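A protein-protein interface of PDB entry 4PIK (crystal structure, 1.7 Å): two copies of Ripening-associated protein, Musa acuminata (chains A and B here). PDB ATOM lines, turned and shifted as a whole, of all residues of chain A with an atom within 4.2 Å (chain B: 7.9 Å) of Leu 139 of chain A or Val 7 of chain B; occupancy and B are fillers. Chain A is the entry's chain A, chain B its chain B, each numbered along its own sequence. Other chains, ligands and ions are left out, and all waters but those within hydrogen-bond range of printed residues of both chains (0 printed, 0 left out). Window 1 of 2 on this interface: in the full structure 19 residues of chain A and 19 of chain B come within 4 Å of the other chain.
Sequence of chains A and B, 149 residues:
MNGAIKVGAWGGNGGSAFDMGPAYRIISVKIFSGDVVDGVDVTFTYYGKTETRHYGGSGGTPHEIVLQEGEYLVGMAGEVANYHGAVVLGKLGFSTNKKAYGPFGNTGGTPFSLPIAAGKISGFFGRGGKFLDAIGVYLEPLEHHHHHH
The backbone NH (N) of Gly 8 of chain B sits at hydrogen-bond distance from the backbone carbonyl oxygen (O) of Pro 115 of chain A, at 2.8 Å.
N of Val 7 of chain A lies within hydrogen-bond range of O of Val 137 of chain A, 2.9 Å away. The side-chain amino group (NZ) of Lys 120 of chain A lies within salt-bridge range of the side-chain carboxylate (OE2) of Glu 140 of chain A (3.3 Å). The backbone carbonyl oxygen of Ile 5 of chain B sits at hydrogen-bond distance from the backbone NH of Leu 139 of chain B, at 2.9 Å. The backbone carbonyl oxygen (O) of Val 7 of chain B sits at hydrogen-bond distance from the backbone NH (N) of Val 137 of chain B (2.9 Å). N of Trp 10 of chain B sits at hydrogen-bond distance from O of Ile 135 of chain B, 2.8 Å away. The backbone carbonyl oxygen of Met 76 of chain B lies within hydrogen-bond range of the backbone NH of Leu 114 of chain B.
Among the printed residues, merely in contact across the chains: Pro 115 of chain A with Val 7 of chain B, Ile 5 of chain A with Ala 118 of chain B, Leu 139 of chain A with Val 7 of chain B, Ile 116 of chain A with Lys 6 of chain B, Pro 115 of chain A with Trp 10 of chain B, Leu 114 of chain A with Leu 114 of chain B, Leu 139 of chain A with Ile 5 of chain B, Val 7 of chain A with Leu 139 of chain B, Glu 140 of chain A with Ile 5 of chain B, Ile 5 of chain A with Leu 139 of chain B, Ile 5 of chain A with Ile 5 of chain B and Pro 115 of chain A with Ala 9 of chain B.
Leu 139 of chain A touches two residues of chain B. Val 7 of chain B touches just these residues of chain A: Pro 115 (3.4 Å) and Leu 139 (3.5 Å). Printed residues of chain A within 4 Å of Leu 139 of chain B: Ile 5 (3.8 Å) and Val 7 (3.7 Å). Of the printed residues of chain A, Trp 10 of chain B touches Pro 115 (3.7 Å). Printed residues of chain B within 4 Å of Pro 115 of chain A: Val 7 (3.4 Å), Gly 8 (2.8 Å), Ala 9 (3.996 Å) and Trp 10 (3.7 Å). Of the printed residues of chain A, Ala 9 of chain B touches Pro 115. Of the printed residues of chain A, Ala 118 of chain B touches Ile 5.
Of the 20 printed residues of chain B, 9 touch a printed residue of chain A. Hydrophobic or aromatic side chains of chain B that line the printed part of chain A: Ile 5, Val 7, Trp 10, Leu 114 and Leu 139. Hydrophobic or aromatic side chains of chain A within 4 Å of the printed part of chain B: Ile 5, Val 7, Leu 114, Pro 115, Ile 116 and Leu 139.
Ile 5 of chain B touches its own counterpart, Ile 5 of chain A. Ile 5 of chain A touches Leu 139 of chain B, and with the chains exchanged Leu 139 of chain A touches Ile 5 of chain B. Val 7 of chain A touches Leu 139 of chain B, and with the chains exchanged Leu 139 of chain A touches Val 7 of chain B. Leu 114 of chain B touches its own counterpart, Leu 114 of chain A. Positions printed for both chains: 5, 7, 114, 116, 121, 137, 138 and 139.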
ATOM      1  N   ILE A   5      23.484   1.634  11.284  1.00  0.00           N
ATOM      2  CA  ILE A   5      23.336   2.098  12.664  1.00  0.00           C
ATOM      3  C   ILE A   5      23.676   0.938  13.556  1.00  0.00           C
ATOM      4  O   ILE A   5      23.001  -0.075  13.500  1.00  0.00           O
ATOM      5  CB  ILE A   5      21.905   2.634  12.979  1.00  0.00           C
ATOM      6  CG1 ILE A   5      21.497   3.776  12.023  1.00  0.00           C
ATOM      7  CG2 ILE A   5      21.797   3.030  14.471  1.00  0.00           C
ATOM      8  CD1 ILE A   5      22.229   5.015  12.215  1.00  0.00           C
ATOM      9  N   VAL A   7      24.557   0.142  17.593  1.00  0.00           N
ATOM     10  CA  VAL A   7      24.646   0.658  18.977  1.00  0.00           C
ATOM     11  C   VAL A   7      25.171  -0.442  19.889  1.00  0.00           C
ATOM     12  O   VAL A   7      24.924  -1.621  19.654  1.00  0.00           O
ATOM     13  CB  VAL A   7      23.344   1.279  19.494  1.00  0.00           C
ATOM     14  CG1 VAL A   7      22.987   2.526  18.677  1.00  0.00           C
ATOM     15  CG2 VAL A   7      22.209   0.271  19.454  1.00  0.00           C
ATOM     16  N   LEU A 114      18.158  -0.826  26.208  1.00  0.00           N
ATOM     17  CA  LEU A 114      17.975  -0.184  24.933  1.00  0.00           C
ATOM     18  C   LEU A 114      16.516  -0.264  24.475  1.00  0.00           C
ATOM     19  O   LEU A 114      16.124  -1.188  23.742  1.00  0.00           O
ATOM     20  CB  LEU A 114      18.909  -0.816  23.874  1.00  0.00           C
ATOM     21  CG  LEU A 114      18.839  -0.134  22.510  1.00  0.00           C
ATOM     22  CD1 LEU A 114      19.599   1.213  22.503  1.00  0.00           C
ATOM     23  CD2 LEU A 114      19.342  -1.081  21.420  1.00  0.00           C
ATOM     24  N   PRO A 115      15.677   0.690  24.921  1.00  0.00           N
ATOM     25  CA  PRO A 115      14.298   0.762  24.405  1.00  0.00           C
ATOM     26  C   PRO A 115      14.337   1.371  23.015  1.00  0.00           C
ATOM     27  O   PRO A 115      15.091   2.336  22.798  1.00  0.00           O
ATOM     28  CB  PRO A 115      13.586   1.719  25.386  1.00  0.00           C
ATOM     29  CG  PRO A 115      14.647   2.182  26.350  1.00  0.00           C
ATOM     30  CD  PRO A 115      15.987   1.813  25.842  1.00  0.00           C
ATOM     31  N   ILE A 116      13.578   0.808  22.072  1.00  0.00           N
ATOM     32  CA  ILE A 116      13.588   1.361  20.699  1.00  0.00           C
ATOM     33  C   ILE A 116      12.206   1.945  20.451  1.00  0.00           C
ATOM     34  O   ILE A 116      11.238   1.202  20.224  1.00  0.00           O
ATOM     35  CB  ILE A 116      14.019   0.317  19.638  1.00  0.00           C
ATOM     36  CG1 ILE A 116      15.397  -0.309  19.999  1.00  0.00           C
ATOM     37  CG2 ILE A 116      14.068   0.946  18.237  1.00  0.00           C
ATOM     38  CD1 ILE A 116      15.534  -1.617  19.427  1.00  0.00           C
ATOM     39  N   LYS A 120      13.700  -1.120  14.793  1.00  0.00           N
ATOM     40  CA  LYS A 120      13.786  -2.511  15.241  1.00  0.00           C
ATOM     41  C   LYS A 120      15.203  -2.992  15.203  1.00  0.00           C
ATOM     42  O   LYS A 120      16.028  -2.456  14.468  1.00  0.00           O
ATOM     43  CB  LYS A 120      12.891  -3.436  14.360  1.00  0.00           C
ATOM     44  CG  LYS A 120      13.321  -3.415  12.892  1.00  0.00           C
ATOM     45  CD  LYS A 120      12.350  -4.191  11.989  1.00  0.00           C
ATOM     46  CE  LYS A 120      12.577  -3.795  10.559  1.00  0.00           C
ATOM     47  NZ  LYS A 120      12.060  -4.803   9.595  1.00  0.00           N
ATOM     48  N   ILE A 121      15.482  -4.065  15.952  1.00  0.00           N
ATOM     49  CA  ILE A 121      16.823  -4.693  15.887  1.00  0.00           C
ATOM     50  C   ILE A 121      16.872  -5.574  14.650  1.00  0.00           C
ATOM     51  O   ILE A 121      15.962  -6.386  14.433  1.00  0.00           O
ATOM     52  CB  ILE A 121      17.056  -5.512  17.168  1.00  0.00           C
ATOM     53  CG1 ILE A 121      17.189  -4.568  18.366  1.00  0.00           C
ATOM     54  CG2 ILE A 121      18.256  -6.470  17.027  1.00  0.00           C
ATOM     55  CD1 ILE A 121      17.142  -5.319  19.741  1.00  0.00           C
ATOM     56  N   VAL A 137      23.790  -4.163  18.721  1.00  0.00           N
ATOM     57  CA  VAL A 137      22.795  -4.425  17.699  1.00  0.00           C
ATOM     58  C   VAL A 137      22.873  -3.463  16.547  1.00  0.00           C
ATOM     59  O   VAL A 137      23.243  -2.290  16.707  1.00  0.00           O
ATOM     60  CB  VAL A 137      21.345  -4.378  18.282  1.00  0.00           C
ATOM     61  CG1 VAL A 137      21.102  -5.521  19.265  1.00  0.00           C
ATOM     62  CG2 VAL A 137      21.065  -3.034  18.967  1.00  0.00           C
ATOM     63  N   TYR A 138      22.372  -3.951  15.394  1.00  0.00           N
ATOM     64  CA  TYR A 138      22.098  -3.147  14.219  1.00  0.00           C
ATOM     65  C   TYR A 138      20.681  -2.689  14.349  1.00  0.00           C
ATOM     66  O   TYR A 138      19.804  -3.494  14.750  1.00  0.00           O
ATOM     67  CB  TYR A 138      22.208  -4.002  12.935  1.00  0.00           C
ATOM     68  CG  TYR A 138      23.638  -4.258  12.510  1.00  0.00           C
ATOM     69  CD1 TYR A 138      24.386  -5.290  13.083  1.00  0.00           C
ATOM     70  CD2 TYR A 138      24.252  -3.459  11.544  1.00  0.00           C
ATOM     71  CE1 TYR A 138      25.698  -5.556  12.657  1.00  0.00           C
ATOM     72  CE2 TYR A 138      25.545  -3.738  11.092  1.00  0.00           C
ATOM     73  CZ  TYR A 138      26.281  -4.751  11.687  1.00  0.00           C
ATOM     74  OH  TYR A 138      27.572  -5.022  11.264  1.00  0.00           O
ATOM     75  N   LEU A 139      20.412  -1.423  13.995  1.00  0.00           N
ATOM     76  CA  LEU A 139      19.039  -0.912  14.046  1.00  0.00           C
ATOM     77  C   LEU A 139      18.582  -0.514  12.665  1.00  0.00           C
ATOM     78  O   LEU A 139      19.391   0.012  11.872  1.00  0.00           O
ATOM     79  CB  LEU A 139      18.918   0.317  14.983  1.00  0.00           C
ATOM     80  CG  LEU A 139      19.289   0.064  16.471  1.00  0.00           C
ATOM     81  CD1 LEU A 139      19.212   1.383  17.282  1.00  0.00           C
ATOM     82  CD2 LEU A 139      18.393  -1.040  17.087  1.00  0.00           C
ATOM     83  N   GLU A 140      17.303  -0.740  12.384  1.00  0.00           N
ATOM     84  CA  GLU A 140      16.726  -0.348  11.113  1.00  0.00           C
ATOM     85  C   GLU A 140      15.384   0.301  11.363  1.00  0.00           C
ATOM     86  O   GLU A 140      14.747   0.056  12.403  1.00  0.00           O
ATOM     87  CB  GLU A 140      16.678  -1.518  10.134  1.00  0.00           C
ATOM     88  CG  GLU A 140      15.811  -2.725  10.407  1.00  0.00           C
ATOM     89  CD  GLU A 140      15.954  -3.769   9.298  1.00  0.00           C
ATOM     90  OE1 GLU A 140      16.750  -3.538   8.357  1.00  0.00           O
ATOM     91  OE2 GLU A 140      15.328  -4.849   9.404  1.00  0.00           O
ATOM     92  N   ALA B   4      12.749   7.326  10.549  1.00  0.00           N
ATOM     93  CA  ALA B   4      13.451   7.700  11.786  1.00  0.00           C
ATOM     94  C   ALA B   4      13.801   6.488  12.623  1.00  0.00           C
ATOM     95  O   ALA B   4      13.099   5.469  12.597  1.00  0.00           O
ATOM     96  CB  ALA B   4      12.556   8.628  12.605  1.00  0.00           C
ATOM     97  N   ILE B   5      14.920   6.597  13.353  1.00  0.00           N
ATOM     98  CA  ILE B   5      15.298   5.619  14.370  1.00  0.00           C
ATOM     99  C   ILE B   5      15.372   6.410  15.684  1.00  0.00           C
ATOM    100  O   ILE B   5      16.184   7.330  15.775  1.00  0.00           O
ATOM    101  CB  ILE B   5      16.605   4.878  14.051  1.00  0.00           C
ATOM    102  CG1 ILE B   5      16.369   3.964  12.814  1.00  0.00           C
ATOM    103  CG2 ILE B   5      17.005   4.048  15.268  1.00  0.00           C
ATOM    104  CD1 ILE B   5      17.577   3.231  12.328  1.00  0.00           C
ATOM    105  N   LYS B   6      14.561   6.012  16.683  1.00  0.00           N
ATOM    106  CA  LYS B   6      14.547   6.694  18.001  1.00  0.00           C
ATOM    107  C   LYS B   6      14.851   5.649  19.055  1.00  0.00           C
ATOM    108  O   LYS B   6      14.181   4.605  19.079  1.00  0.00           O
ATOM    109  CB  LYS B   6      13.156   7.294  18.276  1.00  0.00           C
ATOM    110  CG  LYS B   6      12.784   8.433  17.323  1.00  0.00           C
ATOM    111  CD  LYS B   6      11.302   8.809  17.414  1.00  0.00           C
ATOM    112  CE  LYS B   6      10.998   9.576  18.674  1.00  0.00           C
ATOM    113  NZ  LYS B   6       9.559   9.984  18.752  1.00  0.00           N
ATOM    114  N   VAL B   7      15.841   5.920  19.911  1.00  0.00           N
ATOM    115  CA  VAL B   7      16.180   5.024  21.021  1.00  0.00           C
ATOM    116  C   VAL B   7      15.998   5.794  22.330  1.00  0.00           C
ATOM    117  O   VAL B   7      16.247   7.005  22.387  1.00  0.00           O
ATOM    118  CB  VAL B   7      17.574   4.351  20.919  1.00  0.00           C
ATOM    119  CG1 VAL B   7      17.628   3.488  19.632  1.00  0.00           C
ATOM    120  CG2 VAL B   7      18.689   5.387  20.889  1.00  0.00           C
ATOM    121  N   GLY B   8      15.582   5.061  23.364  1.00  0.00           N
ATOM    122  CA  GLY B   8      15.170   5.669  24.624  1.00  0.00           C
ATOM    123  C   GLY B   8      13.644   5.782  24.613  1.00  0.00           C
ATOM    124  O   GLY B   8      12.968   5.113  23.822  1.00  0.00           O
ATOM    125  N   ALA B   9      13.045   6.592  25.467  1.00  0.00           N
ATOM    126  CA  ALA B   9      13.781   7.452  26.394  1.00  0.00           C
ATOM    127  C   ALA B   9      14.158   6.711  27.653  1.00  0.00           C
ATOM    128  O   ALA B   9      13.574   5.671  27.975  1.00  0.00           O
ATOM    129  CB  ALA B   9      12.917   8.665  26.759  1.00  0.00           C
ATOM    130  N   TRP B  10      15.211   7.192  28.297  1.00  0.00           N
ATOM    131  CA  TRP B  10      15.633   6.689  29.602  1.00  0.00           C
ATOM    132  C   TRP B  10      15.152   7.667  30.621  1.00  0.00           C
ATOM    133  O   TRP B  10      15.301   8.867  30.390  1.00  0.00           O
ATOM    134  CB  TRP B  10      17.151   6.573  29.662  1.00  0.00           C
ATOM    135  CG  TRP B  10      17.673   5.448  28.819  1.00  0.00           C
ATOM    136  CD1 TRP B  10      17.829   4.141  29.193  1.00  0.00           C
ATOM    137  CD2 TRP B  10      18.114   5.536  27.460  1.00  0.00           C
ATOM    138  NE1 TRP B  10      18.362   3.414  28.156  1.00  0.00           N
ATOM    139  CE2 TRP B  10      18.498   4.235  27.060  1.00  0.00           C
ATOM    140  CE3 TRP B  10      18.205   6.591  26.526  1.00  0.00           C
ATOM    141  CZ2 TRP B  10      19.042   3.975  25.795  1.00  0.00           C
ATOM    142  CZ3 TRP B  10      18.657   6.317  25.243  1.00  0.00           C
ATOM    143  CH2 TRP B  10      19.100   5.031  24.896  1.00  0.00           C
ATOM    144  N   MET B  76      25.831   8.776  24.626  1.00  0.00           N
ATOM    145  CA  MET B  76      25.077   9.406  25.719  1.00  0.00           C
ATOM    146  C   MET B  76      25.040   8.424  26.862  1.00  0.00           C
ATOM    147  O   MET B  76      24.901   7.225  26.627  1.00  0.00           O
ATOM    148  CB  MET B  76      23.670   9.793  25.253  1.00  0.00           C
ATOM    149  CG  MET B  76      22.813  10.506  26.354  1.00  0.00           C
ATOM    150  SD  MET B  76      21.197  11.062  25.704  1.00  0.00           S
ATOM    151  CE  MET B  76      20.333   9.503  25.527  1.00  0.00           C
ATOM    152  N   LEU B 114      24.640   4.590  26.138  1.00  0.00           N
ATOM    153  CA  LEU B 114      24.393   4.441  24.717  1.00  0.00           C
ATOM    154  C   LEU B 114      25.666   4.667  23.936  1.00  0.00           C
ATOM    155  O   LEU B 114      25.911   5.766  23.422  1.00  0.00           O
ATOM    156  CB  LEU B 114      23.243   5.340  24.197  1.00  0.00           C
ATOM    157  CG  LEU B 114      22.890   5.196  22.704  1.00  0.00           C
ATOM    158  CD1 LEU B 114      22.185   3.847  22.407  1.00  0.00           C
ATOM    159  CD2 LEU B 114      22.071   6.392  22.238  1.00  0.00           C
ATOM    160  N   ILE B 116      27.661   4.381  20.582  1.00  0.00           N
ATOM    161  CA  ILE B 116      27.204   4.282  19.181  1.00  0.00           C
ATOM    162  C   ILE B 116      28.417   3.869  18.370  1.00  0.00           C
ATOM    163  O   ILE B 116      29.310   4.690  18.122  1.00  0.00           O
ATOM    164  CB  ILE B 116      26.525   5.575  18.639  1.00  0.00           C
ATOM    165  CG1 ILE B 116      25.389   6.065  19.578  1.00  0.00           C
ATOM    166  CG2 ILE B 116      25.975   5.318  17.204  1.00  0.00           C
ATOM    167  CD1 ILE B 116      24.925   7.406  19.308  1.00  0.00           C
ATOM    168  N   ALA B 118      28.436   2.815  15.180  1.00  0.00           N
ATOM    169  CA  ALA B 118      28.305   3.414  13.843  1.00  0.00           C
ATOM    170  C   ALA B 118      27.051   4.263  13.855  1.00  0.00           C
ATOM    171  O   ALA B 118      25.970   3.761  14.165  1.00  0.00           O
ATOM    172  CB  ALA B 118      28.235   2.332  12.755  1.00  0.00           C
ATOM    173  N   ILE B 121      24.028  11.017  16.958  1.00  0.00           N
ATOM    174  CA  ILE B 121      22.779  11.582  17.458  1.00  0.00           C
ATOM    175  C   ILE B 121      22.362  12.738  16.552  1.00  0.00           C
ATOM    176  O   ILE B 121      23.141  13.668  16.300  1.00  0.00           O
ATOM    177  CB  ILE B 121      22.961  12.022  18.930  1.00  0.00           C
ATOM    178  CG1 ILE B 121      23.090  10.751  19.804  1.00  0.00           C
ATOM    179  CG2 ILE B 121      21.747  12.900  19.355  1.00  0.00           C
ATOM    180  CD1 ILE B 121      23.688  11.006  21.256  1.00  0.00           C
ATOM    181  N   GLY B 123      18.964  14.252  16.978  1.00  0.00           N
ATOM    182  CA  GLY B 123      17.877  14.993  17.595  1.00  0.00           C
ATOM    183  C   GLY B 123      17.507  14.355  18.911  1.00  0.00           C
ATOM    184  O   GLY B 123      18.068  13.322  19.279  1.00  0.00           O
ATOM    185  N   PHE B 124      16.595  15.008  19.646  1.00  0.00           N
ATOM    186  CA  PHE B 124      16.195  14.588  20.968  1.00  0.00           C
ATOM    187  C   PHE B 124      14.706  14.519  21.152  1.00  0.00           C
ATOM    188  O   PHE B 124      13.939  15.238  20.509  1.00  0.00           O
ATOM    189  CB  PHE B 124      16.724  15.624  22.010  1.00  0.00           C
ATOM    190  CG  PHE B 124      18.228  15.631  22.107  1.00  0.00           C
ATOM    191  CD1 PHE B 124      18.895  14.655  22.838  1.00  0.00           C
ATOM    192  CD2 PHE B 124      18.978  16.623  21.475  1.00  0.00           C
ATOM    193  CE1 PHE B 124      20.303  14.667  22.937  1.00  0.00           C
ATOM    194  CE2 PHE B 124      20.377  16.653  21.599  1.00  0.00           C
ATOM    195  CZ  PHE B 124      21.027  15.667  22.321  1.00  0.00           C
ATOM    196  N   PHE B 125      14.297  13.673  22.113  1.00  0.00           N
ATOM    197  CA  PHE B 125      12.917  13.629  22.578  1.00  0.00           C
ATOM    198  C   PHE B 125      13.011  13.232  24.056  1.00  0.00           C
ATOM    199  O   PHE B 125      14.098  12.910  24.539  1.00  0.00           O
ATOM    200  CB  PHE B 125      12.056  12.673  21.737  1.00  0.00           C
ATOM    201  CG  PHE B 125      12.438  11.214  21.861  1.00  0.00           C
ATOM    202  CD1 PHE B 125      13.476  10.679  21.093  1.00  0.00           C
ATOM    203  CD2 PHE B 125      11.764  10.381  22.742  1.00  0.00           C
ATOM    204  CE1 PHE B 125      13.830   9.324  21.211  1.00  0.00           C
ATOM    205  CE2 PHE B 125      12.105   9.027  22.853  1.00  0.00           C
ATOM    206  CZ  PHE B 125      13.133   8.508  22.078  1.00  0.00           C
ATOM    207  N   ILE B 135      15.078  11.274  28.656  1.00  0.00           N
ATOM    208  CA  ILE B 135      15.695  11.722  27.398  1.00  0.00           C
ATOM    209  C   ILE B 135      15.901  10.546  26.476  1.00  0.00           C
ATOM    210  O   ILE B 135      16.259   9.458  26.923  1.00  0.00           O
ATOM    211  CB  ILE B 135      17.032  12.493  27.662  1.00  0.00           C
ATOM    212  CG1 ILE B 135      17.461  13.268  26.384  1.00  0.00           C
ATOM    213  CG2 ILE B 135      18.170  11.570  28.216  1.00  0.00           C
ATOM    214  CD1 ILE B 135      18.630  14.392  26.564  1.00  0.00           C
ATOM    215  N   GLY B 136      15.708  10.795  25.195  1.00  0.00           N
ATOM    216  CA  GLY B 136      15.927   9.819  24.134  1.00  0.00           C
ATOM    217  C   GLY B 136      16.540  10.538  22.943  1.00  0.00           C
ATOM    218  O   GLY B 136      16.588  11.778  22.914  1.00  0.00           O
ATOM    219  N   VAL B 137      17.060   9.770  21.964  1.00  0.00           N
ATOM    220  CA  VAL B 137      17.734  10.406  20.818  1.00  0.00           C
ATOM    221  C   VAL B 137      17.308   9.781  19.509  1.00  0.00           C
ATOM    222  O   VAL B 137      16.893   8.618  19.475  1.00  0.00           O
ATOM    223  CB  VAL B 137      19.289  10.330  20.921  1.00  0.00           C
ATOM    224  CG1 VAL B 137      19.821  11.161  22.106  1.00  0.00           C
ATOM    225  CG2 VAL B 137      19.791   8.894  21.023  1.00  0.00           C
ATOM    226  N   TYR B 138      17.337  10.585  18.456  1.00  0.00           N
ATOM    227  CA  TYR B 138      17.203  10.155  17.048  1.00  0.00           C
ATOM    228  C   TYR B 138      18.585   9.812  16.578  1.00  0.00           C
ATOM    229  O   TYR B 138      19.538  10.488  16.990  1.00  0.00           O
ATOM    230  CB  TYR B 138      16.676  11.291  16.167  1.00  0.00           C
ATOM    231  CG  TYR B 138      15.206  11.560  16.326  1.00  0.00           C
ATOM    232  CD1 TYR B 138      14.729  12.328  17.389  1.00  0.00           C
ATOM    233  CD2 TYR B 138      14.291  11.092  15.394  1.00  0.00           C
ATOM    234  CE1 TYR B 138      13.367  12.627  17.516  1.00  0.00           C
ATOM    235  CE2 TYR B 138      12.930  11.377  15.507  1.00  0.00           C
ATOM    236  CZ  TYR B 138      12.470  12.142  16.574  1.00  0.00           C
ATOM    237  OH  TYR B 138      11.117  12.357  16.721  1.00  0.00           O
ATOM    238  N   LEU B 139      18.729   8.764  15.737  1.00  0.00           N
ATOM    239  CA  LEU B 139      20.051   8.377  15.254  1.00  0.00           C
ATOM    240  C   LEU B 139      20.102   8.465  13.755  1.00  0.00           C
ATOM    241  O   LEU B 139      19.091   8.301  13.087  1.00  0.00           O
ATOM    242  CB  LEU B 139      20.373   6.910  15.659  1.00  0.00           C
ATOM    243  CG  LEU B 139      20.408   6.646  17.165  1.00  0.00           C
ATOM    244  CD1 LEU B 139      20.641   5.170  17.434  1.00  0.00           C
ATOM    245  CD2 LEU B 139      21.502   7.509  17.845  1.00  0.00           C
